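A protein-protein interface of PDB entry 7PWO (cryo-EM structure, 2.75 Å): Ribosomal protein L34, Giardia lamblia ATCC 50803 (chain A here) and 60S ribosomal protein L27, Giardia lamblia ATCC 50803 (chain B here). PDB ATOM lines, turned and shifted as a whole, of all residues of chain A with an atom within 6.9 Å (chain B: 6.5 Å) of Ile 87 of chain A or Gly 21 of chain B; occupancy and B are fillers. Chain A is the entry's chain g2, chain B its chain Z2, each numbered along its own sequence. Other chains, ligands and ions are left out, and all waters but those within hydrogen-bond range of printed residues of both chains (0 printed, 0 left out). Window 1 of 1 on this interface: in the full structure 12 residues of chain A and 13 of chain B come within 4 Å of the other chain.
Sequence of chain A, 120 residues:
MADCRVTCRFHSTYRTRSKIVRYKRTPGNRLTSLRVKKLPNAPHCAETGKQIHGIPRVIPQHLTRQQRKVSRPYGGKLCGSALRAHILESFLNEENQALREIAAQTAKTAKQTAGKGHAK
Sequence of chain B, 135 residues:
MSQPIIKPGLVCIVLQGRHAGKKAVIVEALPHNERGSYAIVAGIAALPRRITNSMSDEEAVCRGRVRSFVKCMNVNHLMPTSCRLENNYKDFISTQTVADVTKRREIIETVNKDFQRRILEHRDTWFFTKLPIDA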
ATOM      1  N   PRO A  73     -23.192 -22.582  21.273  1.00  0.00           N
ATOM      2  CA  PRO A  73     -21.856 -23.176  21.424  1.00  0.00           C
ATOM      3  C   PRO A  73     -20.773 -22.114  21.295  1.00  0.00           C
ATOM      4  O   PRO A  73     -20.762 -21.331  20.342  1.00  0.00           O
ATOM      5  CB  PRO A  73     -21.802 -24.194  20.284  1.00  0.00           C
ATOM      6  CG  PRO A  73     -23.215 -24.561  20.059  1.00  0.00           C
ATOM      7  CD  PRO A  73     -24.028 -23.349  20.331  1.00  0.00           C
ATOM      8  N   GLY A  80     -19.606 -15.462  16.911  1.00  0.00           N
ATOM      9  CA  GLY A  80     -20.653 -16.008  16.068  1.00  0.00           C
ATOM     10  C   GLY A  80     -20.279 -16.024  14.606  1.00  0.00           C
ATOM     11  O   GLY A  80     -20.435 -17.047  13.941  1.00  0.00           O
ATOM     12  N   ALA A  82     -17.078 -15.827  14.007  1.00  0.00           N
ATOM     13  CA  ALA A  82     -15.950 -16.719  14.222  1.00  0.00           C
ATOM     14  C   ALA A  82     -16.412 -18.162  14.355  1.00  0.00           C
ATOM     15  O   ALA A  82     -15.770 -19.077  13.829  1.00  0.00           O
ATOM     16  CB  ALA A  82     -15.166 -16.284  15.459  1.00  0.00           C
ATOM     17  N   LEU A  83     -17.526 -18.388  15.055  1.00  0.00           N
ATOM     18  CA  LEU A  83     -18.047 -19.742  15.174  1.00  0.00           C
ATOM     19  C   LEU A  83     -18.417 -20.301  13.808  1.00  0.00           C
ATOM     20  O   LEU A  83     -18.023 -21.419  13.463  1.00  0.00           O
ATOM     21  CB  LEU A  83     -19.243 -19.775  16.127  1.00  0.00           C
ATOM     22  CG  LEU A  83     -19.948 -21.129  16.249  1.00  0.00           C
ATOM     23  CD1 LEU A  83     -19.140 -22.081  17.128  1.00  0.00           C
ATOM     24  CD2 LEU A  83     -21.330 -20.951  16.813  1.00  0.00           C
ATOM     25  N   ARG A  84     -19.153 -19.524  13.007  1.00  0.00           N
ATOM     26  CA  ARG A  84     -19.480 -19.928  11.643  1.00  0.00           C
ATOM     27  C   ARG A  84     -18.232 -20.291  10.845  1.00  0.00           C
ATOM     28  O   ARG A  84     -18.198 -21.308  10.140  1.00  0.00           O
ATOM     29  CB  ARG A  84     -20.237 -18.803  10.947  1.00  0.00           C
ATOM     30  CG  ARG A  84     -20.893 -19.198   9.649  1.00  0.00           C
ATOM     31  CD  ARG A  84     -21.673 -18.039   9.081  1.00  0.00           C
ATOM     32  NE  ARG A  84     -22.180 -18.311   7.749  1.00  0.00           N
ATOM     33  CZ  ARG A  84     -21.447 -18.234   6.644  1.00  0.00           C
ATOM     34  NH1 ARG A  84     -20.173 -17.887   6.717  1.00  0.00           N
ATOM     35  NH2 ARG A  84     -21.987 -18.504   5.464  1.00  0.00           N
ATOM     36  N   ALA A  85     -17.198 -19.454  10.935  1.00  0.00           N
ATOM     37  CA  ALA A  85     -15.970 -19.719  10.197  1.00  0.00           C
ATOM     38  C   ALA A  85     -15.316 -21.017  10.651  1.00  0.00           C
ATOM     39  O   ALA A  85     -14.800 -21.778   9.827  1.00  0.00           O
ATOM     40  CB  ALA A  85     -15.008 -18.541  10.346  1.00  0.00           C
ATOM     41  N   HIS A  86     -15.322 -21.290  11.957  1.00  0.00           N
ATOM     42  CA  HIS A  86     -14.746 -22.540  12.447  1.00  0.00           C
ATOM     43  C   HIS A  86     -15.529 -23.758  11.961  1.00  0.00           C
ATOM     44  O   HIS A  86     -14.931 -24.767  11.565  1.00  0.00           O
ATOM     45  CB  HIS A  86     -14.666 -22.537  13.971  1.00  0.00           C
ATOM     46  CG  HIS A  86     -13.467 -21.832  14.514  1.00  0.00           C
ATOM     47  ND1 HIS A  86     -12.232 -22.435  14.608  1.00  0.00           N
ATOM     48  CD2 HIS A  86     -13.319 -20.588  15.027  1.00  0.00           C
ATOM     49  CE1 HIS A  86     -11.370 -21.584  15.134  1.00  0.00           C
ATOM     50  NE2 HIS A  86     -12.004 -20.457  15.400  1.00  0.00           N
ATOM     51  N   ILE A  87     -16.862 -23.694  12.001  1.00  0.00           N
ATOM     52  CA  ILE A  87     -17.674 -24.815  11.523  1.00  0.00           C
ATOM     53  C   ILE A  87     -17.396 -25.085  10.051  1.00  0.00           C
ATOM     54  O   ILE A  87     -17.219 -26.240   9.635  1.00  0.00           O
ATOM     55  CB  ILE A  87     -19.173 -24.562  11.775  1.00  0.00           C
ATOM     56  CG1 ILE A  87     -19.409 -23.947  13.149  1.00  0.00           C
ATOM     57  CG2 ILE A  87     -19.985 -25.830  11.613  1.00  0.00           C
ATOM     58  CD1 ILE A  87     -20.831 -23.484  13.370  1.00  0.00           C
ATOM     59  N   LEU A  88     -17.354 -24.022   9.242  1.00  0.00           N
ATOM     60  CA  LEU A  88     -17.081 -24.199   7.819  1.00  0.00           C
ATOM     61  C   LEU A  88     -15.696 -24.786   7.593  1.00  0.00           C
ATOM     62  O   LEU A  88     -15.532 -25.702   6.782  1.00  0.00           O
ATOM     63  CB  LEU A  88     -17.221 -22.871   7.075  1.00  0.00           C
ATOM     64  CG  LEU A  88     -18.547 -22.582   6.377  1.00  0.00           C
ATOM     65  CD1 LEU A  88     -19.679 -22.698   7.354  1.00  0.00           C
ATOM     66  CD2 LEU A  88     -18.552 -21.204   5.745  1.00  0.00           C
ATOM     67  N   GLU A  89     -14.683 -24.267   8.295  1.00  0.00           N
ATOM     68  CA  GLU A  89     -13.336 -24.811   8.163  1.00  0.00           C
ATOM     69  C   GLU A  89     -13.316 -26.302   8.446  1.00  0.00           C
ATOM     70  O   GLU A  89     -12.820 -27.094   7.638  1.00  0.00           O
ATOM     71  CB  GLU A  89     -12.372 -24.098   9.105  1.00  0.00           C
ATOM     72  CG  GLU A  89     -11.932 -22.742   8.664  1.00  0.00           C
ATOM     73  CD  GLU A  89     -10.631 -22.788   7.912  1.00  0.00           C
ATOM     74  OE1 GLU A  89     -10.381 -21.877   7.101  1.00  0.00           O
ATOM     75  OE2 GLU A  89      -9.866 -23.749   8.124  1.00  0.00           O
ATOM     76  N   SER A  90     -13.870 -26.705   9.594  1.00  0.00           N
ATOM     77  CA  SER A  90     -13.838 -28.113   9.975  1.00  0.00           C
ATOM     78  C   SER A  90     -14.524 -28.988   8.929  1.00  0.00           C
ATOM     79  O   SER A  90     -13.944 -29.972   8.447  1.00  0.00           O
ATOM     80  CB  SER A  90     -14.481 -28.292  11.350  1.00  0.00           C
ATOM     81  OG  SER A  90     -14.846 -29.638  11.588  1.00  0.00           O
ATOM     82  N   PHE A  91     -15.750 -28.629   8.537  1.00  0.00           N
ATOM     83  CA  PHE A  91     -16.496 -29.484   7.616  1.00  0.00           C
ATOM     84  C   PHE A  91     -15.833 -29.558   6.243  1.00  0.00           C
ATOM     85  O   PHE A  91     -15.651 -30.651   5.687  1.00  0.00           O
ATOM     86  CB  PHE A  91     -17.930 -28.991   7.467  1.00  0.00           C
ATOM     87  CG  PHE A  91     -18.655 -29.631   6.330  1.00  0.00           C
ATOM     88  CD1 PHE A  91     -18.893 -30.996   6.329  1.00  0.00           C
ATOM     89  CD2 PHE A  91     -19.069 -28.882   5.243  1.00  0.00           C
ATOM     90  CE1 PHE A  91     -19.547 -31.592   5.274  1.00  0.00           C
ATOM     91  CE2 PHE A  91     -19.730 -29.474   4.192  1.00  0.00           C
ATOM     92  CZ  PHE A  91     -19.965 -30.831   4.204  1.00  0.00           C
ATOM     93  N   LEU A  92     -15.482 -28.409   5.665  1.00  0.00           N
ATOM     94  CA  LEU A  92     -14.927 -28.430   4.317  1.00  0.00           C
ATOM     95  C   LEU A  92     -13.556 -29.084   4.289  1.00  0.00           C
ATOM     96  O   LEU A  92     -13.200 -29.727   3.295  1.00  0.00           O
ATOM     97  CB  LEU A  92     -14.844 -27.016   3.753  1.00  0.00           C
ATOM     98  CG  LEU A  92     -16.142 -26.337   3.344  1.00  0.00           C
ATOM     99  CD1 LEU A  92     -15.917 -24.839   3.262  1.00  0.00           C
ATOM    100  CD2 LEU A  92     -16.648 -26.885   2.021  1.00  0.00           C
ATOM    101  N   ASN A  93     -12.770 -28.942   5.356  1.00  0.00           N
ATOM    102  CA  ASN A  93     -11.478 -29.611   5.376  1.00  0.00           C
ATOM    103  C   ASN A  93     -11.644 -31.117   5.496  1.00  0.00           C
ATOM    104  O   ASN A  93     -10.887 -31.872   4.880  1.00  0.00           O
ATOM    105  CB  ASN A  93     -10.616 -29.053   6.506  1.00  0.00           C
ATOM    106  CG  ASN A  93     -10.074 -27.673   6.192  1.00  0.00           C
ATOM    107  OD1 ASN A  93     -10.245 -27.168   5.079  1.00  0.00           O
ATOM    108  ND2 ASN A  93      -9.415 -27.053   7.172  1.00  0.00           N
ATOM    109  N   ILE B  13     -25.607 -28.895   7.890  1.00  0.00           N
ATOM    110  CA  ILE B  13     -24.955 -28.470   9.124  1.00  0.00           C
ATOM    111  C   ILE B  13     -25.629 -27.168   9.543  1.00  0.00           C
ATOM    112  O   ILE B  13     -25.892 -26.305   8.698  1.00  0.00           O
ATOM    113  CB  ILE B  13     -23.446 -28.251   8.912  1.00  0.00           C
ATOM    114  CG1 ILE B  13     -22.733 -29.508   8.403  1.00  0.00           C
ATOM    115  CG2 ILE B  13     -22.784 -27.866  10.225  1.00  0.00           C
ATOM    116  CD1 ILE B  13     -22.778 -30.700   9.301  1.00  0.00           C
ATOM    117  N   VAL B  14     -25.946 -27.032  10.828  1.00  0.00           N
ATOM    118  CA  VAL B  14     -26.556 -25.804  11.329  1.00  0.00           C
ATOM    119  C   VAL B  14     -25.456 -24.797  11.632  1.00  0.00           C
ATOM    120  O   VAL B  14     -24.407 -25.149  12.183  1.00  0.00           O
ATOM    121  CB  VAL B  14     -27.422 -26.094  12.571  1.00  0.00           C
ATOM    122  CG1 VAL B  14     -27.969 -24.825  13.144  1.00  0.00           C
ATOM    123  CG2 VAL B  14     -28.557 -27.051  12.231  1.00  0.00           C
ATOM    124  N   LEU B  15     -25.686 -23.533  11.276  1.00  0.00           N
ATOM    125  CA  LEU B  15     -24.650 -22.507  11.333  1.00  0.00           C
ATOM    126  C   LEU B  15     -24.872 -21.452  12.410  1.00  0.00           C
ATOM    127  O   LEU B  15     -23.898 -20.971  12.988  1.00  0.00           O
ATOM    128  CB  LEU B  15     -24.520 -21.817   9.970  1.00  0.00           C
ATOM    129  CG  LEU B  15     -23.845 -22.632   8.865  1.00  0.00           C
ATOM    130  CD1 LEU B  15     -23.641 -21.805   7.618  1.00  0.00           C
ATOM    131  CD2 LEU B  15     -22.535 -23.199   9.345  1.00  0.00           C
ATOM    132  N   GLN B  16     -26.111 -21.064  12.695  1.00  0.00           N
ATOM    133  CA  GLN B  16     -26.412 -20.060  13.709  1.00  0.00           C
ATOM    134  C   GLN B  16     -27.438 -20.611  14.701  1.00  0.00           C
ATOM    135  O   GLN B  16     -28.048 -21.659  14.476  1.00  0.00           O
ATOM    136  CB  GLN B  16     -26.909 -18.761  13.051  1.00  0.00           C
ATOM    137  CG  GLN B  16     -26.215 -18.451  11.719  1.00  0.00           C
ATOM    138  CD  GLN B  16     -26.227 -16.979  11.328  1.00  0.00           C
ATOM    139  OE1 GLN B  16     -26.891 -16.160  11.949  1.00  0.00           O
ATOM    140  NE2 GLN B  16     -25.481 -16.647  10.283  1.00  0.00           N
ATOM    141  N   HIS B  19     -28.304 -24.385  18.114  1.00  0.00           N
ATOM    142  CA  HIS B  19     -27.837 -25.678  17.633  1.00  0.00           C
ATOM    143  C   HIS B  19     -26.784 -25.546  16.539  1.00  0.00           C
ATOM    144  O   HIS B  19     -26.706 -26.391  15.648  1.00  0.00           O
ATOM    145  CB  HIS B  19     -29.006 -26.544  17.155  1.00  0.00           C
ATOM    146  CG  HIS B  19     -30.253 -26.395  17.975  1.00  0.00           C
ATOM    147  ND1 HIS B  19     -31.381 -25.755  17.511  1.00  0.00           N
ATOM    148  CD2 HIS B  19     -30.544 -26.802  19.233  1.00  0.00           C
ATOM    149  CE1 HIS B  19     -32.311 -25.769  18.449  1.00  0.00           C
ATOM    150  NE2 HIS B  19     -31.829 -26.402  19.502  1.00  0.00           N
ATOM    151  N   ALA B  20     -25.950 -24.512  16.610  1.00  0.00           N
ATOM    152  CA  ALA B  20     -24.929 -24.294  15.594  1.00  0.00           C
ATOM    153  C   ALA B  20     -23.921 -25.436  15.573  1.00  0.00           C
ATOM    154  O   ALA B  20     -23.533 -25.965  16.615  1.00  0.00           O
ATOM    155  CB  ALA B  20     -24.212 -22.971  15.841  1.00  0.00           C
ATOM    156  N   GLY B  21     -23.483 -25.804  14.374  1.00  0.00           N
ATOM    157  CA  GLY B  21     -22.565 -26.917  14.217  1.00  0.00           C
ATOM    158  C   GLY B  21     -23.140 -28.270  14.565  1.00  0.00           C
ATOM    159  O   GLY B  21     -22.414 -29.130  15.065  1.00  0.00           O
ATOM    160  N   LYS B  22     -24.433 -28.479  14.325  1.00  0.00           N
ATOM    161  CA  LYS B  22     -25.103 -29.749  14.567  1.00  0.00           C
ATOM    162  C   LYS B  22     -25.785 -30.194  13.283  1.00  0.00           C
ATOM    163  O   LYS B  22     -26.194 -29.368  12.468  1.00  0.00           O
ATOM    164  CB  LYS B  22     -26.127 -29.611  15.692  1.00  0.00           C
ATOM    165  CG  LYS B  22     -25.506 -29.356  17.054  1.00  0.00           C
ATOM    166  CD  LYS B  22     -26.566 -29.249  18.125  1.00  0.00           C
ATOM    167  CE  LYS B  22     -25.966 -28.971  19.481  1.00  0.00           C
ATOM    168  NZ  LYS B  22     -27.030 -28.857  20.506  1.00  0.00           N
ATOM    169  N   LYS B  23     -25.914 -31.503  13.093  1.00  0.00           N
ATOM    170  CA  LYS B  23     -26.427 -32.036  11.837  1.00  0.00           C
ATOM    171  C   LYS B  23     -27.938 -32.198  11.901  1.00  0.00           C
ATOM    172  O   LYS B  23     -28.486 -32.587  12.934  1.00  0.00           O
ATOM    173  CB  LYS B  23     -25.769 -33.376  11.512  1.00  0.00           C
ATOM    174  CG  LYS B  23     -24.263 -33.341  11.586  1.00  0.00           C
ATOM    175  CD  LYS B  23     -23.641 -34.589  11.025  1.00  0.00           C
ATOM    176  CE  LYS B  23     -22.227 -34.735  11.522  1.00  0.00           C
ATOM    177  NZ  LYS B  23     -21.221 -34.227  10.554  1.00  0.00           N
ATOM    178  N   LYS B 130     -20.373 -36.787  15.706  1.00  0.00           N
ATOM    179  CA  LYS B 130     -20.171 -35.392  16.077  1.00  0.00           C
ATOM    180  C   LYS B 130     -19.039 -34.771  15.263  1.00  0.00           C
ATOM    181  O   LYS B 130     -18.007 -35.404  15.027  1.00  0.00           O
ATOM    182  CB  LYS B 130     -19.869 -35.279  17.573  1.00  0.00           C
ATOM    183  CG  LYS B 130     -19.687 -33.857  18.063  1.00  0.00           C
ATOM    184  CD  LYS B 130     -19.519 -33.760  19.566  1.00  0.00           C
ATOM    185  CE  LYS B 130     -18.152 -34.256  20.018  1.00  0.00           C
ATOM    186  NZ  LYS B 130     -17.916 -34.058  21.477  1.00  0.00           N
ATOM    187  N   LEU B 131     -19.249 -33.510  14.814  1.00  0.00           N
ATOM    188  CA  LEU B 131     -18.301 -32.739  14.003  1.00  0.00           C
ATOM    189  C   LEU B 131     -17.282 -32.053  14.908  1.00  0.00           C
ATOM    190  O   LEU B 131     -17.670 -31.442  15.906  1.00  0.00           O
ATOM    191  CB  LEU B 131     -19.031 -31.702  13.160  1.00  0.00           C
ATOM    192  CG  LEU B 131     -18.236 -30.822  12.187  1.00  0.00           C
ATOM    193  CD1 LEU B 131     -17.558 -31.630  11.097  1.00  0.00           C
ATOM    194  CD2 LEU B 131     -19.116 -29.738  11.589  1.00  0.00           C
ATOM    195  N   ILE B 133     -14.862 -29.315  16.248  1.00  0.00           N
ATOM    196  CA  ILE B 133     -14.705 -27.868  16.106  1.00  0.00           C
ATOM    197  C   ILE B 133     -13.506 -27.383  16.917  1.00  0.00           C
ATOM    198  O   ILE B 133     -13.209 -27.895  17.999  1.00  0.00           O
ATOM    199  CB  ILE B 133     -15.974 -27.099  16.545  1.00  0.00           C
ATOM    200  CG1 ILE B 133     -17.177 -27.461  15.681  1.00  0.00           C
ATOM    201  CG2 ILE B 133     -15.764 -25.602  16.483  1.00  0.00           C
ATOM    202  CD1 ILE B 133     -18.158 -28.368  16.349  1.00  0.00           C
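The backbone carbonyl oxygen of Val 14 of chain B lies within hydrogen-bond range of the backbone NH of Gly 21 of chain B, at 2.5 Å.
Pro 73 of chain A touches Ala 20 of chain B (CG to O, 3.7 Å).
CB of Ala 20 of chain B touches CD2 of Leu 83 of chain A, 3.7 Å away.
Leu 15 of chain B touches Arg 84 of chain A (CD1 to NE, 3.8 Å).
CG2 of Ile 87 of chain A touches CG2 of Ile 13 of chain B, 3.7 Å away.
O of Leu 15 of chain B touches CD1 of Ile 87 of chain A, at 3.98 Å.
N of Gly 21 of chain B touches CD1 of Ile 87 of chain A (3.7 Å).
Leu 88 of chain A touches Leu 15 of chain B.
Ser 90 of chain A touches Leu 131 of chain B.
Printed residues of chain B within 4 Å of Leu 83 of chain A: Ala 20.
Printed residues of chain B within 4 Å of Ile 87 of chain A: Ile 13 (3.7 Å), Leu 15 (3.98 Å) and Gly 21 (3.7 Å).
Of the printed residues of chain B, Ser 90 of chain A touches Leu 131.
Phe 91 of chain A touches none of the printed residues of chain B.
Of the printed residues of chain A, Leu 15 of chain B touches Arg 84 (3.8 Å), Ile 87 (3.98 Å) and Leu 88 (3.5 Å).
His 19 of chain B touches none of the printed residues of chain A.
Printed residues of chain A within 4 Å of Leu 131 of chain B: Ser 90 (3.4 Å).
The nearest printed residue of chain B that does not touch Ile 87 of chain A is Leu 131 of chain B (4.004 Å).
The nearest printed residue of chain A that does not touch Gly 21 of chain B is Pro 73 of chain A (5.8 Å).
Of the 12 printed residues of chain B, 5 touch a printed residue of chain A.
Along chain B the printed residues that touch a printed residue of chain A span positions 13 to 131.
Hydrophobic or aromatic side chains of chain A within 4 Å of the printed part of chain B: Pro 73, Leu 83, Ile 87 and Leu 88.
Among the printed residues, no Asp or Glu carboxylate lies within 4 Å of a Lys or Arg side-chain nitrogen of the other chain.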
